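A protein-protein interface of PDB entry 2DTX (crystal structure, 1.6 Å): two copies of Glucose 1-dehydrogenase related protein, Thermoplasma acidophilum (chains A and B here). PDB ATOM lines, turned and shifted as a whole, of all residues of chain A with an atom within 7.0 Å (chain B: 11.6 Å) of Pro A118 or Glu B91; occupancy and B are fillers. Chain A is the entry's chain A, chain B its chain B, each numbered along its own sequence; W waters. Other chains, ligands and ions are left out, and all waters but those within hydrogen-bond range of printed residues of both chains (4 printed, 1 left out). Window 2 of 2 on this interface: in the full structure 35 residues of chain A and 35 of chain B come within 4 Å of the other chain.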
ATOM      1  N   PHE A  69      -9.182 -42.612  14.687  1.00  0.00           N
ATOM      2  CA  PHE A  69      -9.487 -42.377  16.089  1.00  0.00           C
ATOM      3  C   PHE A  69     -10.830 -42.995  16.459  1.00  0.00           C
ATOM      4  O   PHE A  69     -10.971 -43.592  17.526  1.00  0.00           O
ATOM      5  CB  PHE A  69      -9.489 -40.886  16.409  1.00  0.00           C
ATOM      6  CG  PHE A  69      -9.719 -40.584  17.865  1.00  0.00           C
ATOM      7  CD1 PHE A  69     -10.989 -40.243  18.328  1.00  0.00           C
ATOM      8  CD2 PHE A  69      -8.669 -40.648  18.767  1.00  0.00           C
ATOM      9  CE1 PHE A  69     -11.202 -39.965  19.679  1.00  0.00           C
ATOM     10  CE2 PHE A  69      -8.868 -40.375  20.119  1.00  0.00           C
ATOM     11  CZ  PHE A  69     -10.140 -40.031  20.575  1.00  0.00           C
ATOM     12  N   TYR A 110       3.163 -31.714   7.880  1.00  0.00           N
ATOM     13  CA  TYR A 110       2.397 -30.675   8.546  1.00  0.00           C
ATOM     14  C   TYR A 110       0.917 -31.093   8.669  1.00  0.00           C
ATOM     15  O   TYR A 110       0.349 -31.021   9.744  1.00  0.00           O
ATOM     16  CB  TYR A 110       2.547 -29.354   7.763  1.00  0.00           C
ATOM     17  CG  TYR A 110       1.520 -28.306   8.094  1.00  0.00           C
ATOM     18  CD1 TYR A 110       0.543 -27.981   7.168  1.00  0.00           C
ATOM     19  CD2 TYR A 110       1.501 -27.656   9.329  1.00  0.00           C
ATOM     20  CE1 TYR A 110      -0.439 -27.032   7.445  1.00  0.00           C
ATOM     21  CE2 TYR A 110       0.506 -26.689   9.619  1.00  0.00           C
ATOM     22  CZ  TYR A 110      -0.451 -26.395   8.663  1.00  0.00           C
ATOM     23  OH  TYR A 110      -1.419 -25.452   8.929  1.00  0.00           O
ATOM     24  N   ALA A 112      -0.542 -34.213   8.439  1.00  0.00           N
ATOM     25  CA  ALA A 112      -0.743 -35.376   9.307  1.00  0.00           C
ATOM     26  C   ALA A 112      -0.571 -34.988  10.770  1.00  0.00           C
ATOM     27  O   ALA A 112      -1.359 -35.404  11.636  1.00  0.00           O
ATOM     28  CB  ALA A 112       0.227 -36.497   8.939  1.00  0.00           C
ATOM     29  N   SER A 113       0.459 -34.198  11.065  1.00  0.00           N
ATOM     30  CA  SER A 113       0.685 -33.769  12.444  1.00  0.00           C
ATOM     31  C   SER A 113      -0.436 -32.887  12.955  1.00  0.00           C
ATOM     32  O   SER A 113      -0.944 -33.079  14.064  1.00  0.00           O
ATOM     33  CB  SER A 113       2.005 -32.998  12.562  1.00  0.00           C
ATOM     34  OG  SER A 113       3.084 -33.815  12.152  1.00  0.00           O
ATOM     35  N   LYS A 114      -0.854 -31.932  12.134  1.00  0.00           N
ATOM     36  CA  LYS A 114      -1.895 -31.010  12.550  1.00  0.00           C
ATOM     37  C   LYS A 114      -3.200 -31.713  12.918  1.00  0.00           C
ATOM     38  O   LYS A 114      -3.860 -31.339  13.899  1.00  0.00           O
ATOM     39  CB  LYS A 114      -2.162 -29.994  11.430  1.00  0.00           C
ATOM     40  CG  LYS A 114      -3.313 -29.047  11.704  1.00  0.00           C
ATOM     41  CD  LYS A 114      -3.494 -28.072  10.537  1.00  0.00           C
ATOM     42  CE  LYS A 114      -4.902 -27.505  10.533  1.00  0.00           C
ATOM     43  NZ  LYS A 114      -5.229 -26.729  11.745  1.00  0.00           N
ATOM     44  N   PHE A 115      -3.577 -32.719  12.139  1.00  0.00           N
ATOM     45  CA  PHE A 115      -4.837 -33.400  12.421  1.00  0.00           C
ATOM     46  C   PHE A 115      -4.726 -34.513  13.443  1.00  0.00           C
ATOM     47  O   PHE A 115      -5.712 -34.818  14.113  1.00  0.00           O
ATOM     48  CB  PHE A 115      -5.477 -33.883  11.116  1.00  0.00           C
ATOM     49  CG  PHE A 115      -5.828 -32.755  10.195  1.00  0.00           C
ATOM     50  CD1 PHE A 115      -5.181 -32.610   8.969  1.00  0.00           C
ATOM     51  CD2 PHE A 115      -6.736 -31.774  10.597  1.00  0.00           C
ATOM     52  CE1 PHE A 115      -5.427 -31.495   8.154  1.00  0.00           C
ATOM     53  CE2 PHE A 115      -6.994 -30.653   9.790  1.00  0.00           C
ATOM     54  CZ  PHE A 115      -6.334 -30.517   8.567  1.00  0.00           C
ATOM     55  N   ALA A 116      -3.537 -35.098  13.608  1.00  0.00           N
ATOM     56  CA  ALA A 116      -3.393 -36.163  14.600  1.00  0.00           C
ATOM     57  C   ALA A 116      -3.186 -35.636  16.013  1.00  0.00           C
ATOM     58  O   ALA A 116      -3.677 -36.234  16.978  1.00  0.00           O
ATOM     59  CB  ALA A 116      -2.236 -37.073  14.242  1.00  0.00           C
ATOM     60  N   ILE A 117      -2.476 -34.516  16.141  1.00  0.00           N
ATOM     61  CA  ILE A 117      -2.163 -33.988  17.466  1.00  0.00           C
ATOM     62  C   ILE A 117      -3.323 -33.848  18.454  1.00  0.00           C
ATOM     63  O   ILE A 117      -3.208 -34.326  19.587  1.00  0.00           O
ATOM     64  CB  ILE A 117      -1.337 -32.661  17.352  1.00  0.00           C
ATOM     65  CG1 ILE A 117       0.115 -33.014  17.001  1.00  0.00           C
ATOM     66  CG2 ILE A 117      -1.390 -31.879  18.661  1.00  0.00           C
ATOM     67  CD1 ILE A 117       0.973 -31.827  16.548  1.00  0.00           C
ATOM     68  N   PRO A 118      -4.449 -33.240  18.049  1.00  0.00           N
ATOM     69  CA  PRO A 118      -5.574 -33.094  18.988  1.00  0.00           C
ATOM     70  C   PRO A 118      -5.995 -34.424  19.607  1.00  0.00           C
ATOM     71  O   PRO A 118      -6.349 -34.480  20.792  1.00  0.00           O
ATOM     72  CB  PRO A 118      -6.674 -32.484  18.121  1.00  0.00           C
ATOM     73  CG  PRO A 118      -5.886 -31.634  17.150  1.00  0.00           C
ATOM     74  CD  PRO A 118      -4.750 -32.580  16.764  1.00  0.00           C
ATOM     75  N   TYR A 119      -5.964 -35.483  18.806  1.00  0.00           N
ATOM     76  CA  TYR A 119      -6.326 -36.811  19.292  1.00  0.00           C
ATOM     77  C   TYR A 119      -5.218 -37.408  20.134  1.00  0.00           C
ATOM     78  O   TYR A 119      -5.473 -38.039  21.158  1.00  0.00           O
ATOM     79  CB  TYR A 119      -6.599 -37.749  18.125  1.00  0.00           C
ATOM     80  CG  TYR A 119      -7.812 -37.371  17.304  1.00  0.00           C
ATOM     81  CD1 TYR A 119      -7.691 -37.038  15.958  1.00  0.00           C
ATOM     82  CD2 TYR A 119      -9.088 -37.393  17.865  1.00  0.00           C
ATOM     83  CE1 TYR A 119      -8.805 -36.744  15.183  1.00  0.00           C
ATOM     84  CE2 TYR A 119     -10.210 -37.099  17.094  1.00  0.00           C
ATOM     85  CZ  TYR A 119     -10.063 -36.782  15.758  1.00  0.00           C
ATOM     86  OH  TYR A 119     -11.175 -36.537  14.980  1.00  0.00           O
ATOM     87  N   MET A 120      -3.977 -37.218  19.691  1.00  0.00           N
ATOM     88  CA  MET A 120      -2.838 -37.763  20.407  1.00  0.00           C
ATOM     89  C   MET A 120      -2.701 -37.265  21.839  1.00  0.00           C
ATOM     90  O   MET A 120      -2.341 -38.038  22.735  1.00  0.00           O
ATOM     91  CB  MET A 120      -1.555 -37.481  19.608  1.00  0.00           C
ATOM     92  CG  MET A 120      -1.522 -38.250  18.307  1.00  0.00           C
ATOM     93  SD  MET A 120      -0.084 -37.916  17.263  1.00  0.00           S
ATOM     94  CE  MET A 120       1.209 -38.789  18.216  1.00  0.00           C
ATOM     95  N   ILE A 121      -2.981 -35.986  22.062  1.00  0.00           N
ATOM     96  CA  ILE A 121      -2.860 -35.434  23.398  1.00  0.00           C
ATOM     97  C   ILE A 121      -3.933 -35.975  24.329  1.00  0.00           C
ATOM     98  O   ILE A 121      -3.906 -35.702  25.526  1.00  0.00           O
ATOM     99  CB  ILE A 121      -2.892 -33.894  23.399  1.00  0.00           C
ATOM    100  CG1 ILE A 121      -4.167 -33.374  22.745  1.00  0.00           C
ATOM    101  CG2 ILE A 121      -1.643 -33.360  22.688  1.00  0.00           C
ATOM    102  CD1 ILE A 121      -4.246 -31.854  22.743  1.00  0.00           C
ATOM    103  N   ARG A 122      -4.871 -36.746  23.782  1.00  0.00           N
ATOM    104  CA  ARG A 122      -5.909 -37.336  24.617  1.00  0.00           C
ATOM    105  C   ARG A 122      -5.404 -38.685  25.142  1.00  0.00           C
ATOM    106  O   ARG A 122      -6.062 -39.343  25.959  1.00  0.00           O
ATOM    107  CB  ARG A 122      -7.216 -37.465  23.826  1.00  0.00           C
ATOM    108  CG  ARG A 122      -7.872 -36.102  23.588  1.00  0.00           C
ATOM    109  CD  ARG A 122      -8.957 -36.124  22.518  1.00  0.00           C
ATOM    110  NE  ARG A 122     -10.097 -36.956  22.884  1.00  0.00           N
ATOM    111  CZ  ARG A 122     -11.196 -37.072  22.144  1.00  0.00           C
ATOM    112  NH1 ARG A 122     -11.299 -36.402  21.007  1.00  0.00           N
ATOM    113  NH2 ARG A 122     -12.184 -37.873  22.528  1.00  0.00           N
ATOM    114  N   SER A 123      -4.224 -39.091  24.674  1.00  0.00           N
ATOM    115  CA  SER A 123      -3.595 -40.333  25.126  1.00  0.00           C
ATOM    116  C   SER A 123      -2.415 -39.995  26.035  1.00  0.00           C
ATOM    117  O   SER A 123      -1.988 -38.841  26.107  1.00  0.00           O
ATOM    118  CB  SER A 123      -3.086 -41.156  23.945  1.00  0.00           C
ATOM    119  OG  SER A 123      -4.116 -41.943  23.389  1.00  0.00           O
ATOM    120  N   ASP A 163       6.234 -26.743  21.181  1.00  0.00           N
ATOM    121  CA  ASP A 163       4.838 -26.327  21.353  1.00  0.00           C
ATOM    122  C   ASP A 163       4.003 -27.275  22.209  1.00  0.00           C
ATOM    123  O   ASP A 163       3.084 -26.834  22.916  1.00  0.00           O
ATOM    124  CB  ASP A 163       4.144 -26.181  20.004  1.00  0.00           C
ATOM    125  CG  ASP A 163       4.547 -24.923  19.248  1.00  0.00           C
ATOM    126  OD1 ASP A 163       5.428 -24.178  19.715  1.00  0.00           O
ATOM    127  OD2 ASP A 163       3.965 -24.698  18.168  1.00  0.00           O
ATOM    128  N   TYR A 164       4.312 -28.567  22.149  1.00  0.00           N
ATOM    129  CA  TYR A 164       3.526 -29.541  22.900  1.00  0.00           C
ATOM    130  C   TYR A 164       4.183 -30.243  24.085  1.00  0.00           C
ATOM    131  O   TYR A 164       3.543 -31.070  24.752  1.00  0.00           O
ATOM    132  CB  TYR A 164       2.916 -30.556  21.928  1.00  0.00           C
ATOM    133  CG  TYR A 164       1.940 -29.896  20.990  1.00  0.00           C
ATOM    134  CD1 TYR A 164       2.351 -29.422  19.744  1.00  0.00           C
ATOM    135  CD2 TYR A 164       0.628 -29.642  21.387  1.00  0.00           C
ATOM    136  CE1 TYR A 164       1.480 -28.708  18.922  1.00  0.00           C
ATOM    137  CE2 TYR A 164      -0.250 -28.926  20.572  1.00  0.00           C
ATOM    138  CZ  TYR A 164       0.185 -28.463  19.347  1.00  0.00           C
ATOM    139  OH  TYR A 164      -0.690 -27.745  18.559  1.00  0.00           O
ATOM    140  N   LEU A 168       3.425 -34.270  24.714  1.00  0.00           N
ATOM    141  CA  LEU A 168       3.743 -35.017  23.515  1.00  0.00           C
ATOM    142  C   LEU A 168       5.175 -34.707  23.108  1.00  0.00           C
ATOM    143  O   LEU A 168       5.610 -33.566  23.217  1.00  0.00           O
ATOM    144  CB  LEU A 168       2.761 -34.609  22.409  1.00  0.00           C
ATOM    145  CG  LEU A 168       2.924 -35.122  20.982  1.00  0.00           C
ATOM    146  CD1 LEU A 168       1.544 -35.145  20.329  1.00  0.00           C
ATOM    147  CD2 LEU A 168       3.900 -34.232  20.198  1.00  0.00           C
ATOM    148  N   SER B  86       3.749 -14.621  12.022  1.00  0.00           N
ATOM    149  CA  SER B  86       2.519 -14.545  12.807  1.00  0.00           C
ATOM    150  C   SER B  86       2.623 -15.752  13.745  1.00  0.00           C
ATOM    151  O   SER B  86       3.387 -16.686  13.476  1.00  0.00           O
ATOM    152  CB  SER B  86       1.250 -14.591  11.927  1.00  0.00           C
ATOM    153  OG  SER B  86       1.249 -15.653  10.998  1.00  0.00           O
ATOM    154  N   TYR B  87       1.870 -15.740  14.837  1.00  0.00           N
ATOM    155  CA  TYR B  87       1.970 -16.793  15.836  1.00  0.00           C
ATOM    156  C   TYR B  87       0.749 -17.682  16.001  1.00  0.00           C
ATOM    157  O   TYR B  87      -0.383 -17.279  15.711  1.00  0.00           O
ATOM    158  CB  TYR B  87       2.321 -16.144  17.184  1.00  0.00           C
ATOM    159  CG  TYR B  87       3.505 -15.204  17.088  1.00  0.00           C
ATOM    160  CD1 TYR B  87       4.807 -15.688  17.148  1.00  0.00           C
ATOM    161  CD2 TYR B  87       3.320 -13.841  16.848  1.00  0.00           C
ATOM    162  CE1 TYR B  87       5.903 -14.840  16.967  1.00  0.00           C
ATOM    163  CE2 TYR B  87       4.397 -12.986  16.660  1.00  0.00           C
ATOM    164  CZ  TYR B  87       5.689 -13.489  16.719  1.00  0.00           C
ATOM    165  OH  TYR B  87       6.744 -12.637  16.505  1.00  0.00           O
ATOM    166  N   GLY B  88       0.990 -18.900  16.474  1.00  0.00           N
ATOM    167  CA  GLY B  88      -0.092 -19.835  16.697  1.00  0.00           C
ATOM    168  C   GLY B  88       0.385 -21.266  16.640  1.00  0.00           C
ATOM    169  O   GLY B  88       1.349 -21.577  15.942  1.00  0.00           O
ATOM    170  N   LYS B  89      -0.275 -22.141  17.388  1.00  0.00           N
ATOM    171  CA  LYS B  89       0.101 -23.536  17.371  1.00  0.00           C
ATOM    172  C   LYS B  89      -0.416 -24.130  16.076  1.00  0.00           C
ATOM    173  O   LYS B  89      -1.360 -23.611  15.478  1.00  0.00           O
ATOM    174  CB  LYS B  89      -0.479 -24.272  18.581  1.00  0.00           C
ATOM    175  CG  LYS B  89       0.308 -24.006  19.858  1.00  0.00           C
ATOM    176  CD  LYS B  89      -0.086 -24.948  20.977  1.00  0.00           C
ATOM    177  CE  LYS B  89       0.805 -24.735  22.186  1.00  0.00           C
ATOM    178  NZ  LYS B  89       0.830 -23.308  22.598  1.00  0.00           N
ATOM    179  N   ILE B  90       0.220 -25.206  15.635  1.00  0.00           N
ATOM    180  CA  ILE B  90      -0.152 -25.875  14.402  1.00  0.00           C
ATOM    181  C   ILE B  90      -1.658 -26.117  14.375  1.00  0.00           C
ATOM    182  O   ILE B  90      -2.272 -26.203  13.309  1.00  0.00           O
ATOM    183  CB  ILE B  90       0.644 -27.206  14.272  1.00  0.00           C
ATOM    184  CG1 ILE B  90       0.405 -27.849  12.913  1.00  0.00           C
ATOM    185  CG2 ILE B  90       0.267 -28.154  15.387  1.00  0.00           C
ATOM    186  CD1 ILE B  90       1.264 -29.091  12.689  1.00  0.00           C
ATOM    187  N   GLU B  91      -2.248 -26.188  15.567  1.00  0.00           N
ATOM    188  CA  GLU B  91      -3.678 -26.424  15.720  1.00  0.00           C
ATOM    189  C   GLU B  91      -4.588 -25.232  15.477  1.00  0.00           C
ATOM    190  O   GLU B  91      -5.683 -25.388  14.935  1.00  0.00           O
ATOM    191  CB  GLU B  91      -3.970 -26.961  17.125  1.00  0.00           C
ATOM    192  CG  GLU B  91      -3.462 -28.349  17.340  1.00  0.00           C
ATOM    193  CD  GLU B  91      -3.764 -29.220  16.148  1.00  0.00           C
ATOM    194  OE1 GLU B  91      -4.901 -29.128  15.633  1.00  0.00           O
ATOM    195  OE2 GLU B  91      -2.872 -29.989  15.727  1.00  0.00           O
ATOM    196  N   SER B  92      -4.146 -24.053  15.895  1.00  0.00           N
ATOM    197  CA  SER B  92      -4.956 -22.847  15.766  1.00  0.00           C
ATOM    198  C   SER B  92      -4.751 -22.062  14.477  1.00  0.00           C
ATOM    199  O   SER B  92      -5.721 -21.612  13.862  1.00  0.00           O
ATOM    200  CB  SER B  92      -4.714 -21.922  16.962  1.00  0.00           C
ATOM    201  OG  SER B  92      -3.400 -21.386  16.936  1.00  0.00           O
ATOM    202  N   MET B  93      -3.496 -21.882  14.072  1.00  0.00           N
ATOM    203  CA  MET B  93      -3.223 -21.132  12.854  1.00  0.00           C
ATOM    204  C   MET B  93      -3.886 -21.821  11.669  1.00  0.00           C
ATOM    205  O   MET B  93      -3.831 -23.047  11.543  1.00  0.00           O
ATOM    206  CB  MET B  93      -1.712 -21.011  12.607  1.00  0.00           C
ATOM    207  CG  MET B  93      -1.372 -20.174  11.363  1.00  0.00           C
ATOM    208  SD  MET B  93       0.403 -19.845  11.126  1.00  0.00           S
ATOM    209  CE  MET B  93       0.647 -18.525  12.276  1.00  0.00           C
ATOM    210  N   SER B  94      -4.521 -21.025  10.809  1.00  0.00           N
ATOM    211  CA  SER B  94      -5.188 -21.563   9.631  1.00  0.00           C
ATOM    212  C   SER B  94      -4.128 -22.117   8.701  1.00  0.00           C
ATOM    213  O   SER B  94      -2.971 -21.668   8.717  1.00  0.00           O
ATOM    214  CB  SER B  94      -5.967 -20.472   8.887  1.00  0.00           C
ATOM    215  OG  SER B  94      -5.090 -19.562   8.229  1.00  0.00           O
ATOM    216  N   MET B  95      -4.521 -23.092   7.895  1.00  0.00           N
ATOM    217  CA  MET B  95      -3.590 -23.681   6.952  1.00  0.00           C
ATOM    218  C   MET B  95      -3.165 -22.615   5.958  1.00  0.00           C
ATOM    219  O   MET B  95      -2.018 -22.599   5.529  1.00  0.00           O
ATOM    220  CB  MET B  95      -4.225 -24.869   6.231  1.00  0.00           C
ATOM    221  CG  MET B  95      -4.489 -26.066   7.156  1.00  0.00           C
ATOM    222  SD  MET B  95      -4.922 -27.546   6.264  1.00  0.00           S
ATOM    223  CE  MET B  95      -6.583 -27.070   5.625  1.00  0.00           C
ATOM    224  N   GLY B  96      -4.088 -21.725   5.597  1.00  0.00           N
ATOM    225  CA  GLY B  96      -3.758 -20.667   4.655  1.00  0.00           C
ATOM    226  C   GLY B  96      -2.664 -19.739   5.159  1.00  0.00           C
ATOM    227  O   GLY B  96      -1.780 -19.359   4.390  1.00  0.00           O
ATOM    228  N   GLU B  97      -2.715 -19.363   6.433  1.00  0.00           N
ATOM    229  CA  GLU B  97      -1.712 -18.470   7.002  1.00  0.00           C
ATOM    230  C   GLU B  97      -0.381 -19.208   7.130  1.00  0.00           C
ATOM    231  O   GLU B  97       0.691 -18.629   6.931  1.00  0.00           O
ATOM    232  CB  GLU B  97      -2.164 -17.958   8.375  1.00  0.00           C
ATOM    233  CG  GLU B  97      -1.205 -16.983   9.053  1.00  0.00           C
ATOM    234  CD  GLU B  97      -0.796 -15.805   8.166  1.00  0.00           C
ATOM    235  OE1 GLU B  97      -1.584 -15.398   7.281  1.00  0.00           O
ATOM    236  OE2 GLU B  97       0.322 -15.274   8.367  1.00  0.00           O
ATOM    237  N   TRP B  98      -0.456 -20.492   7.449  1.00  0.00           N
ATOM    238  CA  TRP B  98       0.765 -21.289   7.595  1.00  0.00           C
ATOM    239  C   TRP B  98       1.464 -21.364   6.239  1.00  0.00           C
ATOM    240  O   TRP B  98       2.687 -21.129   6.141  1.00  0.00           O
ATOM    241  CB  TRP B  98       0.406 -22.700   8.086  1.00  0.00           C
ATOM    242  CG  TRP B  98       1.516 -23.394   8.855  1.00  0.00           C
ATOM    243  CD1 TRP B  98       1.716 -23.365  10.214  1.00  0.00           C
ATOM    244  CD2 TRP B  98       2.547 -24.232   8.314  1.00  0.00           C
ATOM    245  NE1 TRP B  98       2.803 -24.134  10.546  1.00  0.00           N
ATOM    246  CE2 TRP B  98       3.333 -24.679   9.404  1.00  0.00           C
ATOM    247  CE3 TRP B  98       2.884 -24.652   7.014  1.00  0.00           C
ATOM    248  CZ2 TRP B  98       4.438 -25.532   9.237  1.00  0.00           C
ATOM    249  CZ3 TRP B  98       3.988 -25.506   6.850  1.00  0.00           C
ATOM    250  CH2 TRP B  98       4.744 -25.929   7.964  1.00  0.00           C
ATOM    251  N   LYS B 141       8.425 -20.561  20.748  1.00  0.00           N
ATOM    252  CA  LYS B 141       7.154 -21.269  20.805  1.00  0.00           C
ATOM    253  C   LYS B 141       6.076 -20.587  19.979  1.00  0.00           C
ATOM    254  O   LYS B 141       6.117 -19.373  19.761  1.00  0.00           O
ATOM    255  CB  LYS B 141       6.706 -21.366  22.274  1.00  0.00           C
ATOM    256  CG  LYS B 141       5.565 -22.345  22.549  1.00  0.00           C
ATOM    257  CD  LYS B 141       5.376 -22.546  24.058  1.00  0.00           C
ATOM    258  CE  LYS B 141       4.243 -23.531  24.357  1.00  0.00           C
ATOM    259  NZ  LYS B 141       4.164 -23.864  25.818  1.00  0.00           N
ATOM    260  N   ASN B 142       5.124 -21.392  19.510  1.00  0.00           N
ATOM    261  CA  ASN B 142       3.995 -20.909  18.717  1.00  0.00           C
ATOM    262  C   ASN B 142       4.416 -20.211  17.448  1.00  0.00           C
ATOM    263  O   ASN B 142       3.757 -19.267  16.994  1.00  0.00           O
ATOM    264  CB  ASN B 142       3.135 -19.973  19.569  1.00  0.00           C
ATOM    265  CG  ASN B 142       2.655 -20.643  20.836  1.00  0.00           C
ATOM    266  OD1 ASN B 142       2.299 -21.816  20.826  1.00  0.00           O
ATOM    267  ND2 ASN B 142       2.645 -19.900  21.934  1.00  0.00           N
ATOM    268  N   ALA B 143       5.503 -20.702  16.858  1.00  0.00           N
ATOM    269  CA  ALA B 143       6.037 -20.113  15.635  1.00  0.00           C
ATOM    270  C   ALA B 143       6.423 -21.179  14.614  1.00  0.00           C
ATOM    271  O   ALA B 143       7.381 -20.994  13.851  1.00  0.00           O
ATOM    272  CB  ALA B 143       7.257 -19.250  15.986  1.00  0.00           C
ATOM    273  N   SER B 144       5.661 -22.273  14.548  1.00  0.00           N
ATOM    274  CA  SER B 144       6.028 -23.359  13.637  1.00  0.00           C
ATOM    275  C   SER B 144       6.231 -22.983  12.177  1.00  0.00           C
ATOM    276  O   SER B 144       7.224 -23.393  11.582  1.00  0.00           O
ATOM    277  CB  SER B 144       5.054 -24.538  13.747  1.00  0.00           C
ATOM    278  OG  SER B 144       3.728 -24.162  13.466  1.00  0.00           O
ATOM    279  N   ALA B 145       5.340 -22.201  11.575  1.00  0.00           N
ATOM    280  CA  ALA B 145       5.568 -21.857  10.167  1.00  0.00           C
ATOM    281  C   ALA B 145       6.844 -21.043   9.991  1.00  0.00           C
ATOM    282  O   ALA B 145       7.628 -21.272   9.058  1.00  0.00           O
ATOM    283  CB  ALA B 145       4.391 -21.058   9.610  1.00  0.00           C
HETATM  284  O   HOH W   1      -5.800 -28.924  13.188  1.00  0.00           O
HETATM  285  O   HOH W   2       2.067 -26.123  17.090  1.00  0.00           O
HETATM  286  O   HOH W   3       3.388 -23.290  15.958  1.00  0.00           O
HETATM  287  O   HOH W   4      -1.531 -24.339  11.352  1.00  0.00           O
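Lys A114 touches just these residues of chain B: Ile B90 (3.4 Å), Glu B91 (2.5 Å), Met B93 (3.9 Å) and Met B95 (3.7 Å).
No residue of chain B comes within 4 Å of Ala A116.
Ile A117 touches just these residues of chain B: Ile B90 (3.9 Å) and Glu B91 (3.5 Å).
No residue of chain B comes within 4 Å of Tyr A119.
No residue of chain B comes within 4 Å of Ile A121.
No residue of chain B comes within 4 Å of Arg A122.
Printed residues of chain A within 4 Å of Lys B89: Asp A163 and Tyr A164.
Printed residues of chain B within 4 Å of Tyr A164: Lys B89 (3.5 Å), Ile B90 (3.3 Å) and Glu B91 (3.1 Å).
Of the printed residues of chain A, Trp B98 touches Tyr A110.
Of the printed residues of chain A, Met B93 touches Lys A114.
The nearest residue of chain B that does not touch Pro A118 is Ile B90 (6.8 Å).
The nearest printed residue of chain A that does not touch Lys B89 is Lys A114 (6.2 Å).
The backbone NH of Gly B88 sits at hydrogen-bond distance from the backbone carbonyl oxygen of Asn B142 (2.8 Å).
The indole nitrogen (NE1) of Trp B98 sits at hydrogen-bond distance from the side-chain hydroxyl (OG) of Ser B144 (3.1 Å).
N of Lys B89 lies within hydrogen-bond range of OG of Ser B92, 3.2 Å away.
The side-chain amide oxygen (OD1) of Asn B142 sits at hydrogen-bond distance from the side-chain amino group (NZ) of Lys B89.
No position is printed for both chains.
Of the 17 pairs that touch across the chains among the printed residues, none has its exchanged pair printed and touching as well.
The backbone carbonyl oxygen (O) of Ile B90 lies within hydrogen-bond range of the side-chain amino group (NZ) of Lys A114, 3.4 Å away.
NZ of Lys A114 sits at hydrogen-bond distance from O of Glu B91 (3.5 Å).
The backbone NH (N) of Asn B142 is in hydrogen-bond range of the side-chain carboxylate (OD1) of Asp A163, at 2.8 Å.
Among the printed residues, merely in contact across the chains: Tyr A164 with Glu B91, Pro A118 with Glu B91, Asp A163 with Lys B89, Tyr A164 with Ile B90, Asp A163 with Lys B141, Tyr A110 with Trp B98, Tyr A110 with Met B95, Tyr A164 with Lys B89, Ile A117 with Glu B91, Tyr A110 with Ile B90, Lys A114 with Met B95, Ile A117 with Ile B90, Lys A114 with Met B93 and Ser A113 with Ile B90.
Water W2 bridges N of Ile B90 and OD2 of Asp A163.
Water W1 lies within hydrogen-bond range of OE1 of Glu B91 and NZ of Lys A114.
Water W4 lies within hydrogen-bond range of O of Met B93, OH of Tyr A110 and O of Ile B90.
Water W3 lies within hydrogen-bond range of OG of Ser B144, O of Gly B88, OD2 of Asp A163 and N of Ala B143.
Along chain B the printed residues that touch a printed residue of chain A span positions 89 to 142.
Printed residues of chain A that touch a printed residue of chain B: Tyr A110, Ser A113, Lys A114, Ile A117, Pro A118, Asp A163 and Tyr A164.
Hydrophobic or aromatic side chains of chain A that line the printed part of chain B: Tyr A110, Ile A117, Pro A118 and Tyr A164.
Among the printed residues, no Asp or Glu carboxylate lies within 4 Å of a Lys or Arg side-chain nitrogen of the other chain.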
